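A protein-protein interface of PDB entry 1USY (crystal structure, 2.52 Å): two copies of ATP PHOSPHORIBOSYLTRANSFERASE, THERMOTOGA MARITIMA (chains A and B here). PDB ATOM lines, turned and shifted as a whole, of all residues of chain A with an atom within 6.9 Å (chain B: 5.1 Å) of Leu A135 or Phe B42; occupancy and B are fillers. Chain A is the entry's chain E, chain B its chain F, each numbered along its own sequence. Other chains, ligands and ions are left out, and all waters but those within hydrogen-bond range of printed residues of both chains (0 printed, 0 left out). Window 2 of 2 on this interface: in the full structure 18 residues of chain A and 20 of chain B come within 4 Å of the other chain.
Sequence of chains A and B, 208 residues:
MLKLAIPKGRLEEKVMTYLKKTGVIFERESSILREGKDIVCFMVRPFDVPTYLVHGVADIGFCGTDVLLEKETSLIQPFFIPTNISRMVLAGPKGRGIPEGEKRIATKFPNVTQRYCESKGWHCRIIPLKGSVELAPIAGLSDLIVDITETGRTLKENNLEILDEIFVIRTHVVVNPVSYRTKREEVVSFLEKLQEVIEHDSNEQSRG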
ATOM      1  N   LEU A 129     -22.023 -17.217  23.052  1.00  0.00           N
ATOM      2  CA  LEU A 129     -20.653 -17.703  23.254  1.00  0.00           C
ATOM      3  C   LEU A 129     -20.078 -17.004  24.458  1.00  0.00           C
ATOM      4  O   LEU A 129     -20.535 -15.934  24.844  1.00  0.00           O
ATOM      5  CB  LEU A 129     -19.771 -17.431  22.022  1.00  0.00           C
ATOM      6  CG  LEU A 129     -20.179 -18.168  20.733  1.00  0.00           C
ATOM      7  CD1 LEU A 129     -19.440 -17.646  19.498  1.00  0.00           C
ATOM      8  CD2 LEU A 129     -20.014 -19.696  20.864  1.00  0.00           C
ATOM      9  N   GLY A 131     -16.987 -15.963  24.498  1.00  0.00           N
ATOM     10  CA  GLY A 131     -15.821 -15.242  24.014  1.00  0.00           C
ATOM     11  C   GLY A 131     -15.438 -15.708  22.621  1.00  0.00           C
ATOM     12  O   GLY A 131     -16.180 -16.509  22.033  1.00  0.00           O
ATOM     13  N   SER A 132     -14.284 -15.223  22.125  1.00  0.00           N
ATOM     14  CA  SER A 132     -13.779 -15.477  20.764  1.00  0.00           C
ATOM     15  C   SER A 132     -14.927 -15.371  19.813  1.00  0.00           C
ATOM     16  O   SER A 132     -15.054 -16.165  18.880  1.00  0.00           O
ATOM     17  CB  SER A 132     -13.153 -16.866  20.610  1.00  0.00           C
ATOM     18  OG  SER A 132     -12.455 -17.230  21.772  1.00  0.00           O
ATOM     19  N   VAL A 133     -15.787 -14.412  20.103  1.00  0.00           N
ATOM     20  CA  VAL A 133     -16.998 -14.199  19.355  1.00  0.00           C
ATOM     21  C   VAL A 133     -16.667 -13.841  17.894  1.00  0.00           C
ATOM     22  O   VAL A 133     -17.400 -14.219  16.984  1.00  0.00           O
ATOM     23  CB  VAL A 133     -17.829 -13.080  20.014  1.00  0.00           C
ATOM     24  CG1 VAL A 133     -19.200 -12.958  19.381  1.00  0.00           C
ATOM     25  CG2 VAL A 133     -17.970 -13.299  21.524  1.00  0.00           C
ATOM     26  N   GLU A 134     -15.551 -13.147  17.676  1.00  0.00           N
ATOM     27  CA  GLU A 134     -15.171 -12.588  16.350  1.00  0.00           C
ATOM     28  C   GLU A 134     -14.874 -13.679  15.317  1.00  0.00           C
ATOM     29  O   GLU A 134     -14.821 -13.450  14.112  1.00  0.00           O
ATOM     30  CB  GLU A 134     -13.962 -11.668  16.502  1.00  0.00           C
ATOM     31  CG  GLU A 134     -13.763 -11.198  17.949  1.00  0.00           C
ATOM     32  CD  GLU A 134     -14.651 -10.014  18.325  1.00  0.00           C
ATOM     33  OE1 GLU A 134     -14.921  -9.160  17.433  1.00  0.00           O
ATOM     34  OE2 GLU A 134     -15.080  -9.927  19.511  1.00  0.00           O
ATOM     35  N   LEU A 135     -14.733 -14.863  15.859  1.00  0.00           N
ATOM     36  CA  LEU A 135     -14.411 -16.099  15.198  1.00  0.00           C
ATOM     37  C   LEU A 135     -15.610 -16.794  14.586  1.00  0.00           C
ATOM     38  O   LEU A 135     -15.456 -17.737  13.810  1.00  0.00           O
ATOM     39  CB  LEU A 135     -13.946 -17.028  16.301  1.00  0.00           C
ATOM     40  CG  LEU A 135     -12.818 -17.999  16.162  1.00  0.00           C
ATOM     41  CD1 LEU A 135     -11.590 -17.370  15.485  1.00  0.00           C
ATOM     42  CD2 LEU A 135     -12.509 -18.471  17.572  1.00  0.00           C
ATOM     43  N   ALA A 136     -16.817 -16.403  14.951  1.00  0.00           N
ATOM     44  CA  ALA A 136     -17.941 -17.226  14.504  1.00  0.00           C
ATOM     45  C   ALA A 136     -18.201 -17.216  12.986  1.00  0.00           C
ATOM     46  O   ALA A 136     -18.484 -18.258  12.420  1.00  0.00           O
ATOM     47  CB  ALA A 136     -19.202 -16.915  15.285  1.00  0.00           C
ATOM     48  N   PRO A 137     -18.134 -16.068  12.325  1.00  0.00           N
ATOM     49  CA  PRO A 137     -18.418 -16.031  10.887  1.00  0.00           C
ATOM     50  C   PRO A 137     -17.403 -16.855  10.103  1.00  0.00           C
ATOM     51  O   PRO A 137     -17.808 -17.524   9.168  1.00  0.00           O
ATOM     52  CB  PRO A 137     -18.353 -14.549  10.541  1.00  0.00           C
ATOM     53  CG  PRO A 137     -17.633 -13.908  11.662  1.00  0.00           C
ATOM     54  CD  PRO A 137     -17.832 -14.738  12.869  1.00  0.00           C
ATOM     55  N   ILE A 138     -16.131 -16.830  10.502  1.00  0.00           N
ATOM     56  CA  ILE A 138     -15.083 -17.610   9.833  1.00  0.00           C
ATOM     57  C   ILE A 138     -15.435 -19.092   9.868  1.00  0.00           C
ATOM     58  O   ILE A 138     -15.289 -19.805   8.859  1.00  0.00           O
ATOM     59  CB  ILE A 138     -13.708 -17.441  10.515  1.00  0.00           C
ATOM     60  CG1 ILE A 138     -13.519 -16.043  11.157  1.00  0.00           C
ATOM     61  CG2 ILE A 138     -12.587 -17.850   9.557  1.00  0.00           C
ATOM     62  CD1 ILE A 138     -13.759 -14.811  10.255  1.00  0.00           C
ATOM     63  N   ALA A 139     -15.873 -19.551  11.041  1.00  0.00           N
ATOM     64  CA  ALA A 139     -16.337 -20.915  11.202  1.00  0.00           C
ATOM     65  C   ALA A 139     -17.753 -20.978  10.640  1.00  0.00           C
ATOM     66  O   ALA A 139     -18.251 -20.035  10.037  1.00  0.00           O
ATOM     67  CB  ALA A 139     -16.294 -21.325  12.657  1.00  0.00           C
ATOM     68  N   GLY A 140     -18.430 -22.080  10.804  1.00  0.00           N
ATOM     69  CA  GLY A 140     -19.755 -22.135  10.232  1.00  0.00           C
ATOM     70  C   GLY A 140     -20.814 -21.334  10.962  1.00  0.00           C
ATOM     71  O   GLY A 140     -21.861 -21.079  10.394  1.00  0.00           O
ATOM     72  N   LEU A 141     -20.525 -20.907  12.186  1.00  0.00           N
ATOM     73  CA  LEU A 141     -21.573 -20.628  13.175  1.00  0.00           C
ATOM     74  C   LEU A 141     -22.502 -19.434  13.028  1.00  0.00           C
ATOM     75  O   LEU A 141     -23.650 -19.508  13.464  1.00  0.00           O
ATOM     76  CB  LEU A 141     -20.990 -20.569  14.576  1.00  0.00           C
ATOM     77  CG  LEU A 141     -20.082 -21.685  15.079  1.00  0.00           C
ATOM     78  CD1 LEU A 141     -19.282 -21.147  16.218  1.00  0.00           C
ATOM     79  CD2 LEU A 141     -20.915 -22.888  15.548  1.00  0.00           C
ATOM     80  N   SER A 142     -22.057 -18.312  12.478  1.00  0.00           N
ATOM     81  CA  SER A 142     -22.997 -17.175  12.392  1.00  0.00           C
ATOM     82  C   SER A 142     -22.781 -16.399  11.117  1.00  0.00           C
ATOM     83  O   SER A 142     -21.819 -16.648  10.392  1.00  0.00           O
ATOM     84  CB  SER A 142     -22.900 -16.264  13.647  1.00  0.00           C
ATOM     85  OG  SER A 142     -22.191 -15.056  13.404  1.00  0.00           O
ATOM     86  N   ILE A 145     -21.978 -10.949  14.132  1.00  0.00           N
ATOM     87  CA  ILE A 145     -21.712 -10.954  15.572  1.00  0.00           C
ATOM     88  C   ILE A 145     -22.191  -9.623  16.197  1.00  0.00           C
ATOM     89  O   ILE A 145     -22.268  -8.614  15.498  1.00  0.00           O
ATOM     90  CB  ILE A 145     -20.199 -11.152  15.801  1.00  0.00           C
ATOM     91  CG1 ILE A 145     -19.420  -9.986  15.191  1.00  0.00           C
ATOM     92  CG2 ILE A 145     -19.701 -12.457  15.164  1.00  0.00           C
ATOM     93  CD1 ILE A 145     -18.323  -9.539  16.037  1.00  0.00           C
ATOM     94  N   ASN A 158      -9.587  -9.811  12.186  1.00  0.00           N
ATOM     95  CA  ASN A 158     -10.379 -10.965  11.745  1.00  0.00           C
ATOM     96  C   ASN A 158     -11.278 -10.676  10.544  1.00  0.00           C
ATOM     97  O   ASN A 158     -12.299 -11.359  10.330  1.00  0.00           O
ATOM     98  CB  ASN A 158     -11.229 -11.492  12.895  1.00  0.00           C
ATOM     99  CG  ASN A 158     -10.395 -12.064  13.983  1.00  0.00           C
ATOM    100  OD1 ASN A 158     -10.162 -11.415  15.000  1.00  0.00           O
ATOM    101  ND2 ASN A 158      -9.902 -13.282  13.776  1.00  0.00           N
ATOM    102  N   LEU A 160     -13.459  -8.299   9.756  1.00  0.00           N
ATOM    103  CA  LEU A 160     -14.842  -7.900  10.053  1.00  0.00           C
ATOM    104  C   LEU A 160     -15.010  -6.374  10.032  1.00  0.00           C
ATOM    105  O   LEU A 160     -14.069  -5.619  10.333  1.00  0.00           O
ATOM    106  CB  LEU A 160     -15.285  -8.434  11.422  1.00  0.00           C
ATOM    107  CG  LEU A 160     -15.794  -9.865  11.728  1.00  0.00           C
ATOM    108  CD1 LEU A 160     -16.184 -10.730  10.532  1.00  0.00           C
ATOM    109  CD2 LEU A 160     -14.776 -10.599  12.558  1.00  0.00           C
ATOM    110  N   LYS B   3      -9.527 -29.158  11.549  1.00  0.00           N
ATOM    111  CA  LYS B   3      -9.792 -27.936  12.310  1.00  0.00           C
ATOM    112  C   LYS B   3      -9.925 -28.303  13.777  1.00  0.00           C
ATOM    113  O   LYS B   3     -10.780 -29.111  14.135  1.00  0.00           O
ATOM    114  CB  LYS B   3     -11.070 -27.218  11.812  1.00  0.00           C
ATOM    115  CG  LYS B   3     -10.975 -26.607  10.352  1.00  0.00           C
ATOM    116  CD  LYS B   3     -12.313 -26.036   9.810  1.00  0.00           C
ATOM    117  CE  LYS B   3     -13.245 -27.160   9.271  1.00  0.00           C
ATOM    118  NZ  LYS B   3     -14.617 -26.712   8.818  1.00  0.00           N
ATOM    119  N   LEU B   4      -9.059 -27.717  14.611  1.00  0.00           N
ATOM    120  CA  LEU B   4      -9.073 -27.907  16.064  1.00  0.00           C
ATOM    121  C   LEU B   4      -9.717 -26.779  16.844  1.00  0.00           C
ATOM    122  O   LEU B   4      -9.632 -25.598  16.459  1.00  0.00           O
ATOM    123  CB  LEU B   4      -7.670 -28.021  16.603  1.00  0.00           C
ATOM    124  CG  LEU B   4      -6.634 -28.871  15.909  1.00  0.00           C
ATOM    125  CD1 LEU B   4      -5.606 -29.215  16.938  1.00  0.00           C
ATOM    126  CD2 LEU B   4      -7.190 -30.134  15.286  1.00  0.00           C
ATOM    127  N   ALA B   5     -10.355 -27.135  17.956  1.00  0.00           N
ATOM    128  CA  ALA B   5     -10.996 -26.123  18.810  1.00  0.00           C
ATOM    129  C   ALA B   5     -10.306 -26.179  20.140  1.00  0.00           C
ATOM    130  O   ALA B   5     -10.626 -27.050  20.936  1.00  0.00           O
ATOM    131  CB  ALA B   5     -12.483 -26.392  18.972  1.00  0.00           C
ATOM    132  N   ILE B   6      -9.329 -25.284  20.342  1.00  0.00           N
ATOM    133  CA  ILE B   6      -8.518 -25.272  21.567  1.00  0.00           C
ATOM    134  C   ILE B   6      -9.137 -24.329  22.610  1.00  0.00           C
ATOM    135  O   ILE B   6      -9.493 -23.203  22.275  1.00  0.00           O
ATOM    136  CB  ILE B   6      -7.025 -24.845  21.312  1.00  0.00           C
ATOM    137  CG1 ILE B   6      -6.405 -25.406  20.000  1.00  0.00           C
ATOM    138  CG2 ILE B   6      -6.163 -25.171  22.526  1.00  0.00           C
ATOM    139  CD1 ILE B   6      -6.466 -26.879  19.805  1.00  0.00           C
ATOM    140  N   ILE B  32      -6.609 -15.505  18.308  1.00  0.00           N
ATOM    141  CA  ILE B  32      -7.890 -16.217  18.358  1.00  0.00           C
ATOM    142  C   ILE B  32      -8.044 -17.252  17.206  1.00  0.00           C
ATOM    143  O   ILE B  32      -8.969 -18.067  17.215  1.00  0.00           O
ATOM    144  CB  ILE B  32      -9.011 -15.113  18.389  1.00  0.00           C
ATOM    145  CG1 ILE B  32      -9.341 -14.713  19.827  1.00  0.00           C
ATOM    146  CG2 ILE B  32     -10.272 -15.491  17.670  1.00  0.00           C
ATOM    147  CD1 ILE B  32      -9.222 -13.198  20.073  1.00  0.00           C
ATOM    148  N   LEU B  33      -7.104 -17.237  16.251  1.00  0.00           N
ATOM    149  CA  LEU B  33      -7.139 -18.088  15.055  1.00  0.00           C
ATOM    150  C   LEU B  33      -5.718 -18.406  14.577  1.00  0.00           C
ATOM    151  O   LEU B  33      -5.030 -17.532  14.031  1.00  0.00           O
ATOM    152  CB  LEU B  33      -7.885 -17.328  13.947  1.00  0.00           C
ATOM    153  CG  LEU B  33      -8.469 -17.902  12.651  1.00  0.00           C
ATOM    154  CD1 LEU B  33      -8.604 -16.776  11.615  1.00  0.00           C
ATOM    155  CD2 LEU B  33      -7.676 -19.042  12.066  1.00  0.00           C
ATOM    156  N   VAL B  40      -5.997 -25.975  11.344  1.00  0.00           N
ATOM    157  CA  VAL B  40      -6.364 -24.652  11.808  1.00  0.00           C
ATOM    158  C   VAL B  40      -6.842 -24.753  13.220  1.00  0.00           C
ATOM    159  O   VAL B  40      -7.440 -25.758  13.599  1.00  0.00           O
ATOM    160  CB  VAL B  40      -7.350 -23.835  10.874  1.00  0.00           C
ATOM    161  CG1 VAL B  40      -7.395 -24.345   9.447  1.00  0.00           C
ATOM    162  CG2 VAL B  40      -8.702 -23.683  11.449  1.00  0.00           C
ATOM    163  N   CYS B  41      -6.540 -23.727  14.004  1.00  0.00           N
ATOM    164  CA  CYS B  41      -6.798 -23.740  15.440  1.00  0.00           C
ATOM    165  C   CYS B  41      -7.733 -22.595  15.817  1.00  0.00           C
ATOM    166  O   CYS B  41      -7.382 -21.434  15.706  1.00  0.00           O
ATOM    167  CB  CYS B  41      -5.476 -23.611  16.198  1.00  0.00           C
ATOM    168  SG  CYS B  41      -4.556 -25.153  16.441  1.00  0.00           S
ATOM    169  N   PHE B  42      -8.947 -22.928  16.222  1.00  0.00           N
ATOM    170  CA  PHE B  42      -9.836 -21.930  16.799  1.00  0.00           C
ATOM    171  C   PHE B  42      -9.515 -21.854  18.303  1.00  0.00           C
ATOM    172  O   PHE B  42      -9.601 -22.859  19.011  1.00  0.00           O
ATOM    173  CB  PHE B  42     -11.315 -22.293  16.543  1.00  0.00           C
ATOM    174  CG  PHE B  42     -11.691 -22.383  15.097  1.00  0.00           C
ATOM    175  CD1 PHE B  42     -12.023 -23.585  14.531  1.00  0.00           C
ATOM    176  CD2 PHE B  42     -11.720 -21.251  14.306  1.00  0.00           C
ATOM    177  CE1 PHE B  42     -12.375 -23.684  13.179  1.00  0.00           C
ATOM    178  CE2 PHE B  42     -12.059 -21.326  12.951  1.00  0.00           C
ATOM    179  CZ  PHE B  42     -12.395 -22.557  12.389  1.00  0.00           C
ATOM    180  N   MET B  43      -9.048 -20.694  18.754  1.00  0.00           N
ATOM    181  CA  MET B  43      -8.775 -20.476  20.180  1.00  0.00           C
ATOM    182  C   MET B  43     -10.057 -19.948  20.828  1.00  0.00           C
ATOM    183  O   MET B  43     -10.271 -18.748  20.905  1.00  0.00           O
ATOM    184  CB  MET B  43      -7.605 -19.506  20.401  1.00  0.00           C
ATOM    185  CG  MET B  43      -6.338 -19.813  19.575  1.00  0.00           C
ATOM    186  SD  MET B  43      -5.735 -21.506  19.822  1.00  0.00           S
ATOM    187  CE  MET B  43      -4.847 -21.324  21.377  1.00  0.00           C
ATOM    188  N   VAL B  44     -10.909 -20.869  21.263  1.00  0.00           N
ATOM    189  CA  VAL B  44     -12.253 -20.553  21.724  1.00  0.00           C
ATOM    190  C   VAL B  44     -12.298 -20.698  23.249  1.00  0.00           C
ATOM    191  O   VAL B  44     -11.332 -21.156  23.846  1.00  0.00           O
ATOM    192  CB  VAL B  44     -13.333 -21.493  21.084  1.00  0.00           C
ATOM    193  CG1 VAL B  44     -13.199 -21.592  19.574  1.00  0.00           C
ATOM    194  CG2 VAL B  44     -13.267 -22.853  21.685  1.00  0.00           C
ATOM    195  N   TYR B  52     -18.546 -26.255  18.856  1.00  0.00           N
ATOM    196  CA  TYR B  52     -17.765 -26.280  17.629  1.00  0.00           C
ATOM    197  C   TYR B  52     -17.703 -27.699  17.063  1.00  0.00           C
ATOM    198  O   TYR B  52     -17.856 -27.913  15.870  1.00  0.00           O
ATOM    199  CB  TYR B  52     -16.384 -25.674  17.842  1.00  0.00           C
ATOM    200  CG  TYR B  52     -16.325 -24.153  17.758  1.00  0.00           C
ATOM    201  CD1 TYR B  52     -16.888 -23.350  18.753  1.00  0.00           C
ATOM    202  CD2 TYR B  52     -15.654 -23.525  16.725  1.00  0.00           C
ATOM    203  CE1 TYR B  52     -16.825 -21.992  18.702  1.00  0.00           C
ATOM    204  CE2 TYR B  52     -15.579 -22.156  16.654  1.00  0.00           C
ATOM    205  CZ  TYR B  52     -16.154 -21.387  17.639  1.00  0.00           C
ATOM    206  OH  TYR B  52     -16.054 -20.007  17.538  1.00  0.00           O
ATOM    207  N   VAL B  57     -17.927 -27.850  12.819  1.00  0.00           N
ATOM    208  CA  VAL B  57     -17.086 -26.723  12.417  1.00  0.00           C
ATOM    209  C   VAL B  57     -15.654 -26.935  12.889  1.00  0.00           C
ATOM    210  O   VAL B  57     -14.717 -26.355  12.327  1.00  0.00           O
ATOM    211  CB  VAL B  57     -17.657 -25.345  12.839  1.00  0.00           C
ATOM    212  CG1 VAL B  57     -18.999 -25.121  12.182  1.00  0.00           C
ATOM    213  CG2 VAL B  57     -17.784 -25.228  14.327  1.00  0.00           C
ATOM    214  N   ALA B  58     -15.496 -27.782  13.900  1.00  0.00           N
ATOM    215  CA  ALA B  58     -14.200 -28.389  14.202  1.00  0.00           C
ATOM    216  C   ALA B  58     -14.311 -29.906  14.198  1.00  0.00           C
ATOM    217  O   ALA B  58     -15.399 -30.467  14.358  1.00  0.00           O
ATOM    218  CB  ALA B  58     -13.673 -27.902  15.513  1.00  0.00           C
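Printed residues of chain A that touch a printed residue of chain B: Ser A132, Leu A135, Gly A140 and Leu A141. Hydrophobic or aromatic side chains of chain A within 4 Å of the printed part of chain B: Leu A135 and Leu A141. Of the 14 printed residues of chain B, 6 touch a printed residue of chain A. Hydrophobic or aromatic side chains of chain B that line the printed part of chain A: Ile B32, Phe B42, Val B44, Tyr B52 and Val B57. Among the printed residues, no Asp or Glu carboxylate lies within 4 Å of a Lys or Arg side-chain nitrogen of the other chain.
The backbone carbonyl oxygen (O) of Ala A136 sits at hydrogen-bond distance from the backbone NH (N) of Leu A141 (3.4 Å). The backbone NH of Ile B6 lies within hydrogen-bond range of the backbone carbonyl oxygen of Phe B42, at 2.8 Å. N of Val B44 sits at hydrogen-bond distance from O of Ile B6 (2.9 Å). O of Ile B32 sits at hydrogen-bond distance from N of Met B43 (3.0 Å). O of Tyr B52 sits at hydrogen-bond distance from N of Val B57 (3.1 Å). O of Tyr B52 sits at hydrogen-bond distance from N of Ala B58 (3.1 Å).
Among the printed residues, merely in contact across the chains: Leu A135 with Ile B32 (3.2 Å), Ser A132 with Val B44 (3.3 Å), Gly A140 with Val B57 (3.4 Å), Leu A141 with Tyr B52 (3.4 Å), Leu A135 with Val B44 (3.8 Å), Leu A135 with Tyr B52 (3.9 Å) and Leu A135 with Phe B42 (3.9 Å).
O of Met B43 is in hydrogen-bond range of OG of Ser A132, 2.8 Å away.
Of the printed residues of chain B, Leu A135 touches Ile B32 (3.2 Å), Phe B42 (3.9 Å), Val B44 (3.8 Å) and Tyr B52 (3.9 Å). Phe B42 touches just one residue of chain A: Leu A135. Of the printed residues of chain A, Val B44 touches Ser A132 and Leu A135. Of the printed residues of chain A, Val B57 touches Gly A140 (3.4 Å). Of the printed residues of chain A, Tyr B52 touches Leu A135 (3.9 Å) and Leu A141 (3.4 Å). Of the printed residues of chain B, Leu A141 touches Tyr B52. Ala A139 touches none of the printed residues of chain B. Ile A145 touches none of the printed residues of chain B. The nearest residue of chain A that does not touch Phe B42 is Ala A139 (4.1 Å). The nearest printed residue of chain A that does not touch Val B44 is Gly A131 (5.6 Å).
No position is printed for both chains.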
